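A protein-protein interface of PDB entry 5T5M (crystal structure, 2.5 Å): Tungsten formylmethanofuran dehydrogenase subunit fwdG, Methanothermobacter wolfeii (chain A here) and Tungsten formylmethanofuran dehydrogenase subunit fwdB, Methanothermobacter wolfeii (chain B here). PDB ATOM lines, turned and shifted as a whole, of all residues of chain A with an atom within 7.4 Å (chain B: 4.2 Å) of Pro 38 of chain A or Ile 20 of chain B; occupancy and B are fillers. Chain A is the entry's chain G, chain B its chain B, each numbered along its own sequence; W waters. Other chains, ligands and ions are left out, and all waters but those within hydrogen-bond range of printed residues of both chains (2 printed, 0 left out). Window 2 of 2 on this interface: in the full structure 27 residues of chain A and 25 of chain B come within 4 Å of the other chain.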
ATOM      1  N   VAL A  19     -15.863  21.031  -1.227  1.00  0.00           N
ATOM      2  CA  VAL A  19     -16.393  22.284  -0.704  1.00  0.00           C
ATOM      3  C   VAL A  19     -15.814  23.467  -1.469  1.00  0.00           C
ATOM      4  O   VAL A  19     -16.527  24.431  -1.784  1.00  0.00           O
ATOM      5  CB  VAL A  19     -16.110  22.399   0.803  1.00  0.00           C
ATOM      6  CG1 VAL A  19     -16.579  23.748   1.320  1.00  0.00           C
ATOM      7  CG2 VAL A  19     -16.789  21.268   1.568  1.00  0.00           C
ATOM      8  N   ILE A  20     -14.510  23.425  -1.763  1.00  0.00           N
ATOM      9  CA  ILE A  20     -13.853  24.548  -2.422  1.00  0.00           C
ATOM     10  C   ILE A  20     -14.235  24.608  -3.894  1.00  0.00           C
ATOM     11  O   ILE A  20     -14.490  25.690  -4.443  1.00  0.00           O
ATOM     12  CB  ILE A  20     -12.328  24.440  -2.243  1.00  0.00           C
ATOM     13  CG1 ILE A  20     -11.953  24.335  -0.757  1.00  0.00           C
ATOM     14  CG2 ILE A  20     -11.636  25.611  -2.906  1.00  0.00           C
ATOM     15  CD1 ILE A  20     -12.661  25.337   0.149  1.00  0.00           C
ATOM     16  N   SER A  29     -19.418  32.279  -0.363  1.00  0.00           N
ATOM     17  CA  SER A  29     -18.393  32.493   0.659  1.00  0.00           C
ATOM     18  C   SER A  29     -17.043  32.824   0.027  1.00  0.00           C
ATOM     19  O   SER A  29     -16.409  31.935  -0.581  1.00  0.00           O
ATOM     20  CB  SER A  29     -18.264  31.268   1.552  1.00  0.00           C
ATOM     21  OG  SER A  29     -17.255  31.482   2.523  1.00  0.00           O
ATOM     22  N   GLU A  31     -14.369  33.069   1.622  1.00  0.00           N
ATOM     23  CA  GLU A  31     -13.412  32.190   2.283  1.00  0.00           C
ATOM     24  C   GLU A  31     -13.319  30.854   1.557  1.00  0.00           C
ATOM     25  O   GLU A  31     -12.222  30.382   1.239  1.00  0.00           O
ATOM     26  CB  GLU A  31     -13.804  31.996   3.750  1.00  0.00           C
ATOM     27  CG  GLU A  31     -13.580  33.235   4.591  1.00  0.00           C
ATOM     28  CD  GLU A  31     -14.138  33.109   5.988  1.00  0.00           C
ATOM     29  OE1 GLU A  31     -15.347  32.823   6.133  1.00  0.00           O
ATOM     30  OE2 GLU A  31     -13.359  33.295   6.943  1.00  0.00           O
ATOM     31  N   VAL A  32     -14.470  30.236   1.275  1.00  0.00           N
ATOM     32  CA  VAL A  32     -14.498  28.994   0.505  1.00  0.00           C
ATOM     33  C   VAL A  32     -13.868  29.205  -0.860  1.00  0.00           C
ATOM     34  O   VAL A  32     -13.046  28.404  -1.317  1.00  0.00           O
ATOM     35  CB  VAL A  32     -15.941  28.484   0.366  1.00  0.00           C
ATOM     36  CG1 VAL A  32     -16.009  27.342  -0.633  1.00  0.00           C
ATOM     37  CG2 VAL A  32     -16.495  28.062   1.722  1.00  0.00           C
ATOM     38  N   GLY A  35     -10.281  28.622  -0.852  1.00  0.00           N
ATOM     39  CA  GLY A  35      -9.758  27.378  -0.333  1.00  0.00           C
ATOM     40  C   GLY A  35      -9.876  27.201   1.162  1.00  0.00           C
ATOM     41  O   GLY A  35      -9.376  26.199   1.689  1.00  0.00           O
ATOM     42  N   LYS A  36     -10.504  28.139   1.859  1.00  0.00           N
ATOM     43  CA  LYS A  36     -10.673  28.065   3.299  1.00  0.00           C
ATOM     44  C   LYS A  36     -12.047  27.512   3.639  1.00  0.00           C
ATOM     45  O   LYS A  36     -13.012  27.688   2.894  1.00  0.00           O
ATOM     46  CB  LYS A  36     -10.517  29.443   3.936  1.00  0.00           C
ATOM     47  CG  LYS A  36      -9.132  30.029   3.842  1.00  0.00           C
ATOM     48  CD  LYS A  36      -9.176  31.474   4.234  1.00  0.00           C
ATOM     49  CE  LYS A  36      -7.796  32.062   4.381  1.00  0.00           C
ATOM     50  NZ  LYS A  36      -7.909  33.467   4.894  1.00  0.00           N
ATOM     51  N   GLY A  37     -12.131  26.837   4.777  1.00  0.00           N
ATOM     52  CA  GLY A  37     -13.414  26.515   5.343  1.00  0.00           C
ATOM     53  C   GLY A  37     -14.072  27.799   5.798  1.00  0.00           C
ATOM     54  O   GLY A  37     -13.394  28.731   6.251  1.00  0.00           O
ATOM     55  N   PRO A  38     -15.397  27.892   5.674  1.00  0.00           N
ATOM     56  CA  PRO A  38     -16.072  29.118   6.105  1.00  0.00           C
ATOM     57  C   PRO A  38     -15.934  29.292   7.604  1.00  0.00           C
ATOM     58  O   PRO A  38     -16.060  28.335   8.369  1.00  0.00           O
ATOM     59  CB  PRO A  38     -17.532  28.894   5.692  1.00  0.00           C
ATOM     60  CG  PRO A  38     -17.704  27.422   5.774  1.00  0.00           C
ATOM     61  CD  PRO A  38     -16.368  26.843   5.309  1.00  0.00           C
ATOM     62  N   THR A  39     -15.628  30.518   8.013  1.00  0.00           N
ATOM     63  CA  THR A  39     -15.697  30.921   9.410  1.00  0.00           C
ATOM     64  C   THR A  39     -16.909  31.802   9.651  1.00  0.00           C
ATOM     65  O   THR A  39     -17.649  31.592  10.611  1.00  0.00           O
ATOM     66  CB  THR A  39     -14.409  31.649   9.814  1.00  0.00           C
ATOM     67  OG1 THR A  39     -13.297  30.755   9.672  1.00  0.00           O
ATOM     68  CG2 THR A  39     -14.475  32.128  11.239  1.00  0.00           C
ATOM     69  N   ASP A  40     -17.120  32.788   8.781  1.00  0.00           N
ATOM     70  CA  ASP A  40     -18.388  33.491   8.732  1.00  0.00           C
ATOM     71  C   ASP A  40     -19.529  32.494   8.562  1.00  0.00           C
ATOM     72  O   ASP A  40     -19.412  31.516   7.821  1.00  0.00           O
ATOM     73  CB  ASP A  40     -18.382  34.488   7.573  1.00  0.00           C
ATOM     74  CG  ASP A  40     -17.393  35.618   7.774  1.00  0.00           C
ATOM     75  OD1 ASP A  40     -17.013  35.886   8.936  1.00  0.00           O
ATOM     76  OD2 ASP A  40     -17.008  36.250   6.768  1.00  0.00           O
ATOM     77  N   ASP A  41     -20.636  32.742   9.268  1.00  0.00           N
ATOM     78  CA  ASP A  41     -21.843  31.941   9.087  1.00  0.00           C
ATOM     79  C   ASP A  41     -22.393  32.206   7.693  1.00  0.00           C
ATOM     80  O   ASP A  41     -22.782  33.334   7.373  1.00  0.00           O
ATOM     81  CB  ASP A  41     -22.890  32.274  10.147  1.00  0.00           C
ATOM     82  CG  ASP A  41     -22.707  31.476  11.418  1.00  0.00           C
ATOM     83  OD1 ASP A  41     -21.921  30.506  11.390  1.00  0.00           O
ATOM     84  OD2 ASP A  41     -23.359  31.808  12.433  1.00  0.00           O
ATOM     85  N   VAL A  42     -22.412  31.170   6.862  1.00  0.00           N
ATOM     86  CA  VAL A  42     -22.946  31.247   5.513  1.00  0.00           C
ATOM     87  C   VAL A  42     -23.711  29.956   5.254  1.00  0.00           C
ATOM     88  O   VAL A  42     -23.446  28.918   5.868  1.00  0.00           O
ATOM     89  CB  VAL A  42     -21.822  31.492   4.474  1.00  0.00           C
ATOM     90  CG1 VAL A  42     -20.525  30.777   4.872  1.00  0.00           C
ATOM     91  CG2 VAL A  42     -22.252  31.052   3.090  1.00  0.00           C
ATOM     92  N   GLU A  43     -24.694  30.034   4.368  1.00  0.00           N
ATOM     93  CA  GLU A  43     -25.528  28.889   4.016  1.00  0.00           C
ATOM     94  C   GLU A  43     -25.015  28.368   2.678  1.00  0.00           C
ATOM     95  O   GLU A  43     -25.233  28.987   1.632  1.00  0.00           O
ATOM     96  CB  GLU A  43     -27.001  29.287   3.960  1.00  0.00           C
ATOM     97  CG  GLU A  43     -27.944  28.428   4.834  1.00  0.00           C
ATOM     98  CD  GLU A  43     -27.749  28.622   6.343  1.00  0.00           C
ATOM     99  OE1 GLU A  43     -27.523  27.618   7.057  1.00  0.00           O
ATOM    100  OE2 GLU A  43     -27.827  29.777   6.816  1.00  0.00           O
ATOM    101  N   ILE A  44     -24.297  27.245   2.715  1.00  0.00           N
ATOM    102  CA  ILE A  44     -23.785  26.630   1.494  1.00  0.00           C
ATOM    103  C   ILE A  44     -24.300  25.198   1.392  1.00  0.00           C
ATOM    104  O   ILE A  44     -25.020  24.720   2.274  1.00  0.00           O
ATOM    105  CB  ILE A  44     -22.246  26.670   1.439  1.00  0.00           C
ATOM    106  CG1 ILE A  44     -21.620  26.110   2.725  1.00  0.00           C
ATOM    107  CG2 ILE A  44     -21.777  28.092   1.166  1.00  0.00           C
ATOM    108  CD1 ILE A  44     -20.103  26.158   2.737  1.00  0.00           C
ATOM    109  N   MET A  46     -22.673  22.198   1.300  1.00  0.00           N
ATOM    110  CA  MET A  46     -22.091  21.224   2.205  1.00  0.00           C
ATOM    111  C   MET A  46     -20.819  21.807   2.790  1.00  0.00           C
ATOM    112  O   MET A  46     -20.258  22.782   2.281  1.00  0.00           O
ATOM    113  CB  MET A  46     -21.805  19.893   1.501  1.00  0.00           C
ATOM    114  CG  MET A  46     -20.665  19.917   0.487  1.00  0.00           C
ATOM    115  SD  MET A  46     -21.113  20.754  -1.053  1.00  0.00           S
ATOM    116  CE  MET A  46     -20.332  19.675  -2.248  1.00  0.00           C
ATOM    117  N   ILE A  47     -20.397  21.202   3.893  1.00  0.00           N
ATOM    118  CA  ILE A  47     -19.144  21.497   4.565  1.00  0.00           C
ATOM    119  C   ILE A  47     -18.535  20.173   4.993  1.00  0.00           C
ATOM    120  O   ILE A  47     -19.139  19.109   4.847  1.00  0.00           O
ATOM    121  CB  ILE A  47     -19.328  22.386   5.809  1.00  0.00           C
ATOM    122  CG1 ILE A  47     -20.414  21.773   6.700  1.00  0.00           C
ATOM    123  CG2 ILE A  47     -19.610  23.812   5.421  1.00  0.00           C
ATOM    124  CD1 ILE A  47     -20.650  22.513   7.985  1.00  0.00           C
ATOM    125  N   VAL A  48     -17.335  20.261   5.551  1.00  0.00           N
ATOM    126  CA  VAL A  48     -16.747  19.174   6.320  1.00  0.00           C
ATOM    127  C   VAL A  48     -17.101  19.426   7.778  1.00  0.00           C
ATOM    128  O   VAL A  48     -16.728  20.459   8.347  1.00  0.00           O
ATOM    129  CB  VAL A  48     -15.227  19.100   6.112  1.00  0.00           C
ATOM    130  CG1 VAL A  48     -14.621  18.018   6.982  1.00  0.00           C
ATOM    131  CG2 VAL A  48     -14.902  18.849   4.637  1.00  0.00           C
ATOM    132  N   ASP A  50     -17.306  17.404  11.635  1.00  0.00           N
ATOM    133  CA  ASP A  50     -16.865  16.227  12.379  1.00  0.00           C
ATOM    134  C   ASP A  50     -15.964  15.348  11.520  1.00  0.00           C
ATOM    135  O   ASP A  50     -15.980  14.120  11.618  1.00  0.00           O
ATOM    136  CB  ASP A  50     -18.063  15.432  12.904  1.00  0.00           C
ATOM    137  CG  ASP A  50     -18.855  16.198  13.949  1.00  0.00           C
ATOM    138  OD1 ASP A  50     -18.265  17.093  14.596  1.00  0.00           O
ATOM    139  OD2 ASP A  50     -20.057  15.906  14.134  1.00  0.00           O
ATOM    140  N   VAL B   4     -15.999  27.686  19.109  1.00  0.00           N
ATOM    141  CA  VAL B   4     -14.683  28.310  19.118  1.00  0.00           C
ATOM    142  C   VAL B   4     -14.176  28.290  17.688  1.00  0.00           C
ATOM    143  O   VAL B   4     -13.865  27.224  17.145  1.00  0.00           O
ATOM    144  CB  VAL B   4     -13.708  27.595  20.059  1.00  0.00           C
ATOM    145  CG1 VAL B   4     -12.423  28.413  20.190  1.00  0.00           C
ATOM    146  CG2 VAL B   4     -14.352  27.346  21.414  1.00  0.00           C
ATOM    147  N   LYS B   5     -14.087  29.466  17.085  1.00  0.00           N
ATOM    148  CA  LYS B   5     -13.646  29.618  15.709  1.00  0.00           C
ATOM    149  C   LYS B   5     -12.206  30.105  15.684  1.00  0.00           C
ATOM    150  O   LYS B   5     -11.671  30.589  16.683  1.00  0.00           O
ATOM    151  CB  LYS B   5     -14.549  30.601  14.955  1.00  0.00           C
ATOM    152  CG  LYS B   5     -16.011  30.165  14.854  1.00  0.00           C
ATOM    153  CD  LYS B   5     -16.832  31.110  13.974  1.00  0.00           C
ATOM    154  CE  LYS B   5     -18.274  30.637  13.814  1.00  0.00           C
ATOM    155  NZ  LYS B   5     -19.081  31.541  12.942  1.00  0.00           N
ATOM    156  N   ASP B  18      -8.264  27.649  10.638  1.00  0.00           N
ATOM    157  CA  ASP B  18      -9.675  27.967  10.438  1.00  0.00           C
ATOM    158  C   ASP B  18     -10.577  26.895  11.043  1.00  0.00           C
ATOM    159  O   ASP B  18     -11.707  26.698  10.590  1.00  0.00           O
ATOM    160  CB  ASP B  18      -9.980  28.123   8.950  1.00  0.00           C
ATOM    161  CG  ASP B  18      -9.697  26.850   8.182  1.00  0.00           C
ATOM    162  OD1 ASP B  18      -8.946  26.016   8.731  1.00  0.00           O
ATOM    163  OD2 ASP B  18     -10.217  26.677   7.055  1.00  0.00           O
ATOM    164  N   ILE B  19     -10.090  26.175  12.045  1.00  0.00           N
ATOM    165  CA  ILE B  19     -10.884  25.117  12.656  1.00  0.00           C
ATOM    166  C   ILE B  19     -11.919  25.741  13.577  1.00  0.00           C
ATOM    167  O   ILE B  19     -11.664  26.755  14.244  1.00  0.00           O
ATOM    168  CB  ILE B  19      -9.988  24.126  13.419  1.00  0.00           C
ATOM    169  CG1 ILE B  19      -8.866  23.586  12.513  1.00  0.00           C
ATOM    170  CG2 ILE B  19     -10.822  22.984  13.970  1.00  0.00           C
ATOM    171  CD1 ILE B  19      -9.336  22.934  11.232  1.00  0.00           C
ATOM    172  N   ILE B  20     -13.101  25.136  13.609  1.00  0.00           N
ATOM    173  CA  ILE B  20     -14.166  25.519  14.522  1.00  0.00           C
ATOM    174  C   ILE B  20     -14.405  24.339  15.453  1.00  0.00           C
ATOM    175  O   ILE B  20     -14.695  23.227  14.989  1.00  0.00           O
ATOM    176  CB  ILE B  20     -15.448  25.895  13.766  1.00  0.00           C
ATOM    177  CG1 ILE B  20     -15.192  27.114  12.867  1.00  0.00           C
ATOM    178  CG2 ILE B  20     -16.611  26.117  14.748  1.00  0.00           C
ATOM    179  CD1 ILE B  20     -16.416  27.576  12.060  1.00  0.00           C
ATOM    180  N   CYS B  21     -14.303  24.579  16.757  1.00  0.00           N
ATOM    181  CA  CYS B  21     -14.450  23.526  17.754  1.00  0.00           C
ATOM    182  C   CYS B  21     -15.811  23.619  18.429  1.00  0.00           C
ATOM    183  O   CYS B  21     -16.236  24.702  18.848  1.00  0.00           O
ATOM    184  CB  CYS B  21     -13.339  23.603  18.802  1.00  0.00           C
ATOM    185  SG  CYS B  21     -11.758  23.007  18.166  1.00  0.00           S
ATOM    186  N   LYS B  22     -16.490  22.479  18.516  1.00  0.00           N
ATOM    187  CA  LYS B  22     -17.741  22.355  19.255  1.00  0.00           C
ATOM    188  C   LYS B  22     -17.398  21.988  20.694  1.00  0.00           C
ATOM    189  O   LYS B  22     -16.887  20.894  20.953  1.00  0.00           O
ATOM    190  CB  LYS B  22     -18.637  21.291  18.626  1.00  0.00           C
ATOM    191  CG  LYS B  22     -19.125  21.592  17.217  1.00  0.00           C
ATOM    192  CD  LYS B  22     -19.793  20.359  16.621  1.00  0.00           C
ATOM    193  CE  LYS B  22     -20.276  20.585  15.197  1.00  0.00           C
ATOM    194  NZ  LYS B  22     -20.644  19.291  14.544  1.00  0.00           N
ATOM    195  N   THR B  31     -15.996  19.052  15.537  1.00  0.00           N
ATOM    196  CA  THR B  31     -15.272  20.117  14.854  1.00  0.00           C
ATOM    197  C   THR B  31     -16.022  20.517  13.590  1.00  0.00           C
ATOM    198  O   THR B  31     -16.949  19.832  13.143  1.00  0.00           O
ATOM    199  CB  THR B  31     -13.844  19.684  14.486  1.00  0.00           C
ATOM    200  OG1 THR B  31     -13.893  18.632  13.513  1.00  0.00           O
ATOM    201  CG2 THR B  31     -13.087  19.198  15.717  1.00  0.00           C
ATOM    202  N   ILE B  32     -15.599  21.642  13.013  1.00  0.00           N
ATOM    203  CA  ILE B  32     -15.961  22.018  11.652  1.00  0.00           C
ATOM    204  C   ILE B  32     -14.681  22.343  10.884  1.00  0.00           C
ATOM    205  O   ILE B  32     -13.709  22.854  11.447  1.00  0.00           O
ATOM    206  CB  ILE B  32     -16.944  23.219  11.613  1.00  0.00           C
ATOM    207  CG1 ILE B  32     -18.141  22.969  12.540  1.00  0.00           C
ATOM    208  CG2 ILE B  32     -17.403  23.484  10.192  1.00  0.00           C
ATOM    209  CD1 ILE B  32     -19.155  24.116  12.591  1.00  0.00           C
ATOM    210  N   ASN B  33     -14.689  22.026   9.587  1.00  0.00           N
ATOM    211  CA  ASN B  33     -13.600  22.334   8.656  1.00  0.00           C
ATOM    212  C   ASN B  33     -12.391  21.402   8.809  1.00  0.00           C
ATOM    213  O   ASN B  33     -11.683  21.145   7.830  1.00  0.00           O
ATOM    214  CB  ASN B  33     -13.167  23.804   8.794  1.00  0.00           C
ATOM    215  CG  ASN B  33     -14.226  24.794   8.256  1.00  0.00           C
ATOM    216  OD1 ASN B  33     -15.060  24.446   7.418  1.00  0.00           O
ATOM    217  ND2 ASN B  33     -14.168  26.033   8.725  1.00  0.00           N
HETATM  218  O   HOH W   1     -14.534  19.003  10.757  1.00  0.00           O
HETATM  219  O   HOH W   2     -12.836  29.049  11.759  1.00  0.00           O
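C of Lys 36 of chain A touches OD2 of Asp 18 of chain B, at 3.96 Å. Asn 33 of chain B touches Gly 37 of chain A. Ile 20 of chain B touches Pro 38 of chain A (CD1 to O, 3.8 Å). Ile 32 of chain B touches Val 48 of chain A (CG2 to O, 3.6 Å).
O of Asp 18 of chain B sits at hydrogen-bond distance from ND2 of Asn 33 of chain B. O of Ile 20 of chain B lies within hydrogen-bond range of N of Ile 32 of chain B, at 2.7 Å. O of Glu 31 of chain A lies within hydrogen-bond range of N of Lys 36 of chain A (2.9 Å). The backbone NH (N) of Thr 39 of chain A lies within hydrogen-bond range of the side-chain carboxylate (OE1) of Glu 31 of chain A.
Of chain A, only Pro 38 comes within 4 Å of Ile 20 of chain B. Of the printed residues of chain B, Thr 39 of chain A touches Lys 5 (2.7 Å). Of the printed residues of chain A, Lys 5 of chain B touches Thr 39 (2.7 Å) and Asp 41 (3.4 Å). Of the printed residues of chain A, Asn 33 of chain B touches Gly 37, Pro 38 and Val 48. Of the printed residues of chain A, Asp 18 of chain B touches Lys 36 (3.96 Å) and Gly 37 (3.0 Å). Printed residues of chain A within 4 Å of Ile 32 of chain B: Val 48. Gly 35 of chain A touches none of the printed residues of chain B. The nearest printed residue of chain B that does not touch Pro 38 of chain A is Asp 18 of chain B (5.2 Å). The nearest residue of chain A that does not touch Ile 20 of chain B is Thr 39 of chain A (4.3 Å). The nearest printed residue of chain A that does not touch Thr 31 of chain B is Val 48 of chain A (4.8 Å).
Water W2 bridges the side-chain hydroxyl (OG1) of Thr 39 of chain A and the backbone carbonyl oxygen (O) of Asp 18 of chain B. Water W1 lies within hydrogen-bond range of OG1 of Thr 31 of chain B (2.9 Å), N of Asn 33 of chain B (3.2 Å) and N of Asp 50 of chain A (3.3 Å).
NZ of Lys 5 of chain B lies within hydrogen-bond range of O of Thr 39 of chain A (2.7 Å). OD1 of Asp 41 of chain A lies within salt-bridge range of NZ of Lys 5 of chain B. The side-chain carboxylate (OD2) of Asp 18 of chain B sits at hydrogen-bond distance from the backbone NH (N) of Gly 37 of chain A (3.0 Å). NZ of Lys 22 of chain B is in salt-bridge range of OD1 of Asp 50 of chain A. The backbone carbonyl oxygen (O) of Thr 31 of chain B is in hydrogen-bond range of the backbone NH (N) of Asp 50 of chain A (2.9 Å). O of Pro 38 of chain A is in hydrogen-bond range of ND2 of Asn 33 of chain B (3.0 Å). N of Asn 33 of chain B is in hydrogen-bond range of O of Val 48 of chain A, at 2.9 Å.
Hydrophobic or aromatic side chains of chain B within 4 Å of the printed part of chain A: Ile 20 and Ile 32. Among the printed residues, Asp or Glu carboxylates within 4 Å of a Lys or Arg side-chain nitrogen of the other chain: Asp 41 of chain A with Lys 5 of chain B and Asp 50 of chain A with Lys 22 of chain B.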
